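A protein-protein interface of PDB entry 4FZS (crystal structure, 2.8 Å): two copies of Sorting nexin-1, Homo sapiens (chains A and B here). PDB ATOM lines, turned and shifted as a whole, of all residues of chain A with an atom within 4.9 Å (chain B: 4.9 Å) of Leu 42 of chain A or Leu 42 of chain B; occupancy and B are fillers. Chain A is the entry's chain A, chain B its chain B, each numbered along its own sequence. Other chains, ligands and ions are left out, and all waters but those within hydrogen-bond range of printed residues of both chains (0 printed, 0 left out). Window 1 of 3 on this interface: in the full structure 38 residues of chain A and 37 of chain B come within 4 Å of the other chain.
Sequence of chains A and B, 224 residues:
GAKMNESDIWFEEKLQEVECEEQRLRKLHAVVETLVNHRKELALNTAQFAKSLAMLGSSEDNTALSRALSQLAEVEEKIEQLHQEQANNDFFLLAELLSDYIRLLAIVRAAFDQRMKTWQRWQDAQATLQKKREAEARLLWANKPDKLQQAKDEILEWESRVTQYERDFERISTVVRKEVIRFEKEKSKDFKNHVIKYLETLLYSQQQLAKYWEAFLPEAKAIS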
ATOM      1  N   HIS A  38      22.662 -20.105  -6.885  1.00  0.00           N
ATOM      2  CA  HIS A  38      22.255 -19.431  -5.665  1.00  0.00           C
ATOM      3  C   HIS A  38      22.194 -17.907  -5.915  1.00  0.00           C
ATOM      4  O   HIS A  38      21.131 -17.328  -5.700  1.00  0.00           O
ATOM      5  CB  HIS A  38      23.204 -19.778  -4.511  1.00  0.00           C
ATOM      6  CG  HIS A  38      22.723 -19.325  -3.169  1.00  0.00           C
ATOM      7  ND1 HIS A  38      21.662 -19.954  -2.529  1.00  0.00           N
ATOM      8  CD2 HIS A  38      23.176 -18.320  -2.383  1.00  0.00           C
ATOM      9  CE1 HIS A  38      21.505 -19.313  -1.380  1.00  0.00           C
ATOM     10  NE2 HIS A  38      22.394 -18.324  -1.246  1.00  0.00           N
ATOM     11  N   ARG A  39      23.282 -17.277  -6.446  1.00  0.00           N
ATOM     12  CA  ARG A  39      23.301 -15.829  -6.731  1.00  0.00           C
ATOM     13  C   ARG A  39      22.364 -15.422  -7.850  1.00  0.00           C
ATOM     14  O   ARG A  39      22.016 -14.238  -7.961  1.00  0.00           O
ATOM     15  CB  ARG A  39      24.708 -15.238  -6.903  1.00  0.00           C
ATOM     16  CG  ARG A  39      24.692 -13.712  -6.730  1.00  0.00           C
ATOM     17  CD  ARG A  39      25.985 -13.128  -6.203  1.00  0.00           C
ATOM     18  NE  ARG A  39      25.895 -12.714  -4.800  1.00  0.00           N
ATOM     19  CZ  ARG A  39      26.678 -13.180  -3.831  1.00  0.00           C
ATOM     20  NH1 ARG A  39      27.606 -14.093  -4.097  1.00  0.00           N
ATOM     21  NH2 ARG A  39      26.538 -12.740  -2.586  1.00  0.00           N
ATOM     22  N   LYS A  40      21.900 -16.403  -8.630  1.00  0.00           N
ATOM     23  CA  LYS A  40      20.910 -16.193  -9.685  1.00  0.00           C
ATOM     24  C   LYS A  40      19.552 -16.027  -9.005  1.00  0.00           C
ATOM     25  O   LYS A  40      18.906 -14.988  -9.168  1.00  0.00           O
ATOM     26  CB  LYS A  40      20.891 -17.402 -10.653  1.00  0.00           C
ATOM     27  CG  LYS A  40      20.145 -17.207 -11.984  1.00  0.00           C
ATOM     28  CD  LYS A  40      20.300 -18.427 -12.917  1.00  0.00           C
ATOM     29  CE  LYS A  40      19.413 -19.604 -12.555  1.00  0.00           C
ATOM     30  NZ  LYS A  40      19.875 -20.870 -13.188  1.00  0.00           N
ATOM     31  N   GLU A  41      19.156 -17.041  -8.219  1.00  0.00           N
ATOM     32  CA  GLU A  41      17.904 -17.096  -7.470  1.00  0.00           C
ATOM     33  C   GLU A  41      17.731 -15.888  -6.527  1.00  0.00           C
ATOM     34  O   GLU A  41      16.675 -15.268  -6.543  1.00  0.00           O
ATOM     35  CB  GLU A  41      17.808 -18.413  -6.711  1.00  0.00           C
ATOM     36  CG  GLU A  41      16.416 -19.009  -6.746  1.00  0.00           C
ATOM     37  CD  GLU A  41      16.266 -20.322  -5.997  1.00  0.00           C
ATOM     38  OE1 GLU A  41      17.268 -20.788  -5.401  1.00  0.00           O
ATOM     39  OE2 GLU A  41      15.144 -20.883  -6.003  1.00  0.00           O
ATOM     40  N   LEU A  42      18.774 -15.521  -5.765  1.00  0.00           N
ATOM     41  CA  LEU A  42      18.725 -14.373  -4.861  1.00  0.00           C
ATOM     42  C   LEU A  42      18.384 -13.073  -5.564  1.00  0.00           C
ATOM     43  O   LEU A  42      17.511 -12.366  -5.077  1.00  0.00           O
ATOM     44  CB  LEU A  42      20.024 -14.187  -4.061  1.00  0.00           C
ATOM     45  CG  LEU A  42      20.304 -15.124  -2.914  1.00  0.00           C
ATOM     46  CD1 LEU A  42      21.579 -14.711  -2.227  1.00  0.00           C
ATOM     47  CD2 LEU A  42      19.180 -15.136  -1.916  1.00  0.00           C
ATOM     48  N   ALA A  43      19.049 -12.742  -6.687  1.00  0.00           N
ATOM     49  CA  ALA A  43      18.743 -11.501  -7.419  1.00  0.00           C
ATOM     50  C   ALA A  43      17.356 -11.586  -8.080  1.00  0.00           C
ATOM     51  O   ALA A  43      16.718 -10.559  -8.332  1.00  0.00           O
ATOM     52  CB  ALA A  43      19.810 -11.225  -8.462  1.00  0.00           C
ATOM     53  N   LEU A  44      16.882 -12.814  -8.323  1.00  0.00           N
ATOM     54  CA  LEU A  44      15.585 -13.024  -8.921  1.00  0.00           C
ATOM     55  C   LEU A  44      14.513 -12.771  -7.892  1.00  0.00           C
ATOM     56  O   LEU A  44      13.722 -11.844  -8.077  1.00  0.00           O
ATOM     57  CB  LEU A  44      15.471 -14.432  -9.506  1.00  0.00           C
ATOM     58  CG  LEU A  44      14.439 -14.574 -10.611  1.00  0.00           C
ATOM     59  CD1 LEU A  44      15.103 -14.521 -11.992  1.00  0.00           C
ATOM     60  CD2 LEU A  44      13.586 -15.817 -10.401  1.00  0.00           C
ATOM     61  N   ASN A  45      14.519 -13.544  -6.782  1.00  0.00           N
ATOM     62  CA  ASN A  45      13.553 -13.412  -5.681  1.00  0.00           C
ATOM     63  C   ASN A  45      13.488 -12.002  -5.135  1.00  0.00           C
ATOM     64  O   ASN A  45      12.391 -11.549  -4.827  1.00  0.00           O
ATOM     65  CB  ASN A  45      13.847 -14.405  -4.558  1.00  0.00           C
ATOM     66  CG  ASN A  45      13.701 -15.854  -4.963  1.00  0.00           C
ATOM     67  OD1 ASN A  45      13.082 -16.199  -5.989  1.00  0.00           O
ATOM     68  ND2 ASN A  45      14.272 -16.740  -4.161  1.00  0.00           N
ATOM     69  N   THR A  46      14.646 -11.302  -5.044  1.00  0.00           N
ATOM     70  CA  THR A  46      14.686  -9.938  -4.527  1.00  0.00           C
ATOM     71  C   THR A  46      13.981  -8.928  -5.466  1.00  0.00           C
ATOM     72  O   THR A  46      13.147  -8.155  -4.986  1.00  0.00           O
ATOM     73  CB  THR A  46      16.041  -9.535  -3.838  1.00  0.00           C
ATOM     74  OG1 THR A  46      17.110  -9.533  -4.771  1.00  0.00           O
ATOM     75  CG2 THR A  46      16.412 -10.444  -2.652  1.00  0.00           C
ATOM     76  N   HIS A  83      23.815  -7.482  -6.059  1.00  0.00           N
ATOM     77  CA  HIS A  83      23.883  -8.890  -6.479  1.00  0.00           C
ATOM     78  C   HIS A  83      24.168  -8.954  -7.997  1.00  0.00           C
ATOM     79  O   HIS A  83      24.797  -9.906  -8.455  1.00  0.00           O
ATOM     80  CB  HIS A  83      22.562  -9.633  -6.191  1.00  0.00           C
ATOM     81  CG  HIS A  83      22.399 -10.137  -4.785  1.00  0.00           C
ATOM     82  ND1 HIS A  83      23.401 -10.861  -4.145  1.00  0.00           N
ATOM     83  CD2 HIS A  83      21.322 -10.067  -3.963  1.00  0.00           C
ATOM     84  CE1 HIS A  83      22.914 -11.173  -2.951  1.00  0.00           C
ATOM     85  NE2 HIS A  83      21.669 -10.713  -2.795  1.00  0.00           N
ATOM     86  N   HIS B  38       8.740 -14.457   1.855  1.00  0.00           N
ATOM     87  CA  HIS B  38      10.108 -14.118   1.520  1.00  0.00           C
ATOM     88  C   HIS B  38      11.058 -14.676   2.585  1.00  0.00           C
ATOM     89  O   HIS B  38      11.967 -15.439   2.237  1.00  0.00           O
ATOM     90  CB  HIS B  38      10.275 -12.615   1.347  1.00  0.00           C
ATOM     91  CG  HIS B  38      11.591 -12.218   0.737  1.00  0.00           C
ATOM     92  ND1 HIS B  38      11.853 -12.411  -0.613  1.00  0.00           N
ATOM     93  CD2 HIS B  38      12.669 -11.630   1.309  1.00  0.00           C
ATOM     94  CE1 HIS B  38      13.080 -11.951  -0.812  1.00  0.00           C
ATOM     95  NE2 HIS B  38      13.606 -11.461   0.314  1.00  0.00           N
ATOM     96  N   ARG B  39      10.812 -14.366   3.874  1.00  0.00           N
ATOM     97  CA  ARG B  39      11.632 -14.875   4.967  1.00  0.00           C
ATOM     98  C   ARG B  39      11.668 -16.423   4.976  1.00  0.00           C
ATOM     99  O   ARG B  39      12.718 -17.018   5.266  1.00  0.00           O
ATOM    100  CB  ARG B  39      11.213 -14.228   6.316  1.00  0.00           C
ATOM    101  CG  ARG B  39      11.524 -15.000   7.596  1.00  0.00           C
ATOM    102  CD  ARG B  39      12.830 -14.636   8.257  1.00  0.00           C
ATOM    103  NE  ARG B  39      13.956 -15.437   7.756  1.00  0.00           N
ATOM    104  CZ  ARG B  39      14.808 -15.032   6.811  1.00  0.00           C
ATOM    105  NH1 ARG B  39      14.671 -13.835   6.247  1.00  0.00           N
ATOM    106  NH2 ARG B  39      15.800 -15.821   6.423  1.00  0.00           N
ATOM    107  N   LYS B  40      10.543 -17.056   4.575  1.00  0.00           N
ATOM    108  CA  LYS B  40      10.376 -18.514   4.514  1.00  0.00           C
ATOM    109  C   LYS B  40      11.343 -19.074   3.462  1.00  0.00           C
ATOM    110  O   LYS B  40      12.197 -19.901   3.788  1.00  0.00           O
ATOM    111  CB  LYS B  40       8.913 -18.856   4.168  1.00  0.00           C
ATOM    112  CG  LYS B  40       8.479 -20.310   4.381  1.00  0.00           C
ATOM    113  CD  LYS B  40       6.973 -20.511   4.107  1.00  0.00           C
ATOM    114  CE  LYS B  40       6.613 -20.600   2.633  1.00  0.00           C
ATOM    115  NZ  LYS B  40       5.161 -20.357   2.391  1.00  0.00           N
ATOM    116  N   GLU B  41      11.236 -18.568   2.222  1.00  0.00           N
ATOM    117  CA  GLU B  41      12.049 -18.945   1.083  1.00  0.00           C
ATOM    118  C   GLU B  41      13.549 -18.749   1.353  1.00  0.00           C
ATOM    119  O   GLU B  41      14.316 -19.673   1.093  1.00  0.00           O
ATOM    120  CB  GLU B  41      11.606 -18.160  -0.150  1.00  0.00           C
ATOM    121  CG  GLU B  41      11.600 -18.979  -1.429  1.00  0.00           C
ATOM    122  CD  GLU B  41      11.219 -18.224  -2.692  1.00  0.00           C
ATOM    123  OE1 GLU B  41      10.982 -16.996  -2.609  1.00  0.00           O
ATOM    124  OE2 GLU B  41      11.175 -18.859  -3.772  1.00  0.00           O
ATOM    125  N   LEU B  42      13.962 -17.595   1.919  1.00  0.00           N
ATOM    126  CA  LEU B  42      15.359 -17.330   2.252  1.00  0.00           C
ATOM    127  C   LEU B  42      15.958 -18.356   3.190  1.00  0.00           C
ATOM    128  O   LEU B  42      17.045 -18.830   2.904  1.00  0.00           O
ATOM    129  CB  LEU B  42      15.580 -15.940   2.832  1.00  0.00           C
ATOM    130  CG  LEU B  42      15.542 -14.768   1.885  1.00  0.00           C
ATOM    131  CD1 LEU B  42      15.862 -13.492   2.639  1.00  0.00           C
ATOM    132  CD2 LEU B  42      16.519 -14.939   0.741  1.00  0.00           C
ATOM    133  N   ALA B  43      15.285 -18.714   4.295  1.00  0.00           N
ATOM    134  CA  ALA B  43      15.824 -19.723   5.217  1.00  0.00           C
ATOM    135  C   ALA B  43      15.815 -21.123   4.569  1.00  0.00           C
ATOM    136  O   ALA B  43      16.606 -21.996   4.943  1.00  0.00           O
ATOM    137  CB  ALA B  43      15.024 -19.740   6.504  1.00  0.00           C
ATOM    138  N   LEU B  44      14.932 -21.317   3.580  1.00  0.00           N
ATOM    139  CA  LEU B  44      14.838 -22.573   2.884  1.00  0.00           C
ATOM    140  C   LEU B  44      16.005 -22.702   1.930  1.00  0.00           C
ATOM    141  O   LEU B  44      16.812 -23.605   2.107  1.00  0.00           O
ATOM    142  CB  LEU B  44      13.506 -22.690   2.157  1.00  0.00           C
ATOM    143  CG  LEU B  44      13.085 -24.126   1.879  1.00  0.00           C
ATOM    144  CD1 LEU B  44      12.083 -24.621   2.929  1.00  0.00           C
ATOM    145  CD2 LEU B  44      12.568 -24.269   0.455  1.00  0.00           C
ATOM    146  N   ASN B  45      16.132 -21.775   0.963  1.00  0.00           N
ATOM    147  CA  ASN B  45      17.215 -21.759  -0.022  1.00  0.00           C
ATOM    148  C   ASN B  45      18.590 -21.777   0.619  1.00  0.00           C
ATOM    149  O   ASN B  45      19.482 -22.452   0.088  1.00  0.00           O
ATOM    150  CB  ASN B  45      17.093 -20.573  -0.966  1.00  0.00           C
ATOM    151  CG  ASN B  45      15.839 -20.582  -1.820  1.00  0.00           C
ATOM    152  OD1 ASN B  45      15.145 -21.602  -1.982  1.00  0.00           O
ATOM    153  ND2 ASN B  45      15.519 -19.433  -2.391  1.00  0.00           N
ATOM    154  N   THR B  46      18.761 -21.085   1.778  1.00  0.00           N
ATOM    155  CA  THR B  46      20.058 -21.045   2.475  1.00  0.00           C
ATOM    156  C   THR B  46      20.434 -22.406   3.081  1.00  0.00           C
ATOM    157  O   THR B  46      21.554 -22.866   2.854  1.00  0.00           O
ATOM    158  CB  THR B  46      20.333 -19.745   3.291  1.00  0.00           C
ATOM    159  OG1 THR B  46      19.399 -19.622   4.340  1.00  0.00           O
ATOM    160  CG2 THR B  46      20.289 -18.463   2.432  1.00  0.00           C
ATOM    161  N   GLU B  80      22.548 -16.948   8.920  1.00  0.00           N
ATOM    162  CA  GLU B  80      21.101 -17.188   8.814  1.00  0.00           C
ATOM    163  C   GLU B  80      20.315 -16.818  10.075  1.00  0.00           C
ATOM    164  O   GLU B  80      19.261 -16.188   9.961  1.00  0.00           O
ATOM    165  CB  GLU B  80      20.776 -18.619   8.388  1.00  0.00           C
ATOM    166  CG  GLU B  80      19.785 -18.682   7.242  1.00  0.00           C
ATOM    167  CD  GLU B  80      18.378 -18.152   7.460  1.00  0.00           C
ATOM    168  OE1 GLU B  80      17.692 -18.628   8.396  1.00  0.00           O
ATOM    169  OE2 GLU B  80      17.934 -17.313   6.644  1.00  0.00           O
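ND2 of Asn 45 of chain A lies close to ND2 of Asn 45 of chain B, 3.5 Å away.
Of chain B, only Leu 42 (3.8 Å) comes within 4 Å of Leu 42 of chain A. Of chain A, only Leu 42 comes within 4 Å of Leu 42 of chain B. Of the printed residues of chain A, Asn 45 of chain B touches Glu 41 (3.7 Å) and Asn 45 (3.5 Å). Printed residues of chain B within 4 Å of Asn 45 of chain A: Glu 41 and Asn 45. Arg 39 of chain B touches none of the printed residues of chain A. Thr 46 of chain A touches none of the printed residues of chain B. The nearest printed residue of chain A that does not touch Leu 42 of chain B is Thr 46 of chain A (5.6 Å). The nearest printed residue of chain B that does not touch Asn 45 of chain A is His 38 of chain B (4.1 Å).
Among the printed residues, merely in contact across the chains: Asn 45 of chain A with Glu 41 of chain B (3.6 Å), Glu 41 of chain A with Asn 45 of chain B (3.7 Å) and Leu 42 of chain A with Leu 42 of chain B (3.8 Å).
Glu 41 of chain A touches Asn 45 of chain B, and with the chains exchanged Asn 45 of chain A touches Glu 41 of chain B. Leu 42 of chain A touches its own counterpart, Leu 42 of chain B. Asn 45 of chain B touches its own counterpart, Asn 45 of chain A. 9 positions are printed for both chains. Of the 4 pairs that touch across the chains among the printed residues, 4 have their exchanged pair printed and touching as well.
Of the 10 printed residues of chain B, 3 touch a printed residue of chain A. Printed residues of chain B that touch a printed residue of chain A: Glu 41, Leu 42 and Asn 45. Hydrophobic or aromatic side chains of chain B that line the printed part of chain A: Leu 42. Of the 10 printed residues of chain A, 3 touch a printed residue of chain B. Hydrophobic or aromatic side chains of chain A within 4 Å of the printed part of chain B: Leu 42. Along chain A the printed residues that touch a printed residue of chain B span positions 41 to 45. Among the printed residues, 4 pairs touch across the chains. Among the printed residues, no Asp or Glu carboxylate lies within 4 Å of a Lys or Arg side-chain nitrogen of the other chain.
The backbone carbonyl oxygen (O) of Leu 42 of chain A sits at hydrogen-bond distance from the side-chain hydroxyl (OG1) of Thr 46 of chain A. The side-chain hydroxyl (OG1) of Thr 46 of chain B is in hydrogen-bond range of the backbone carbonyl oxygen (O) of Leu 42 of chain B, at 2.9 Å.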
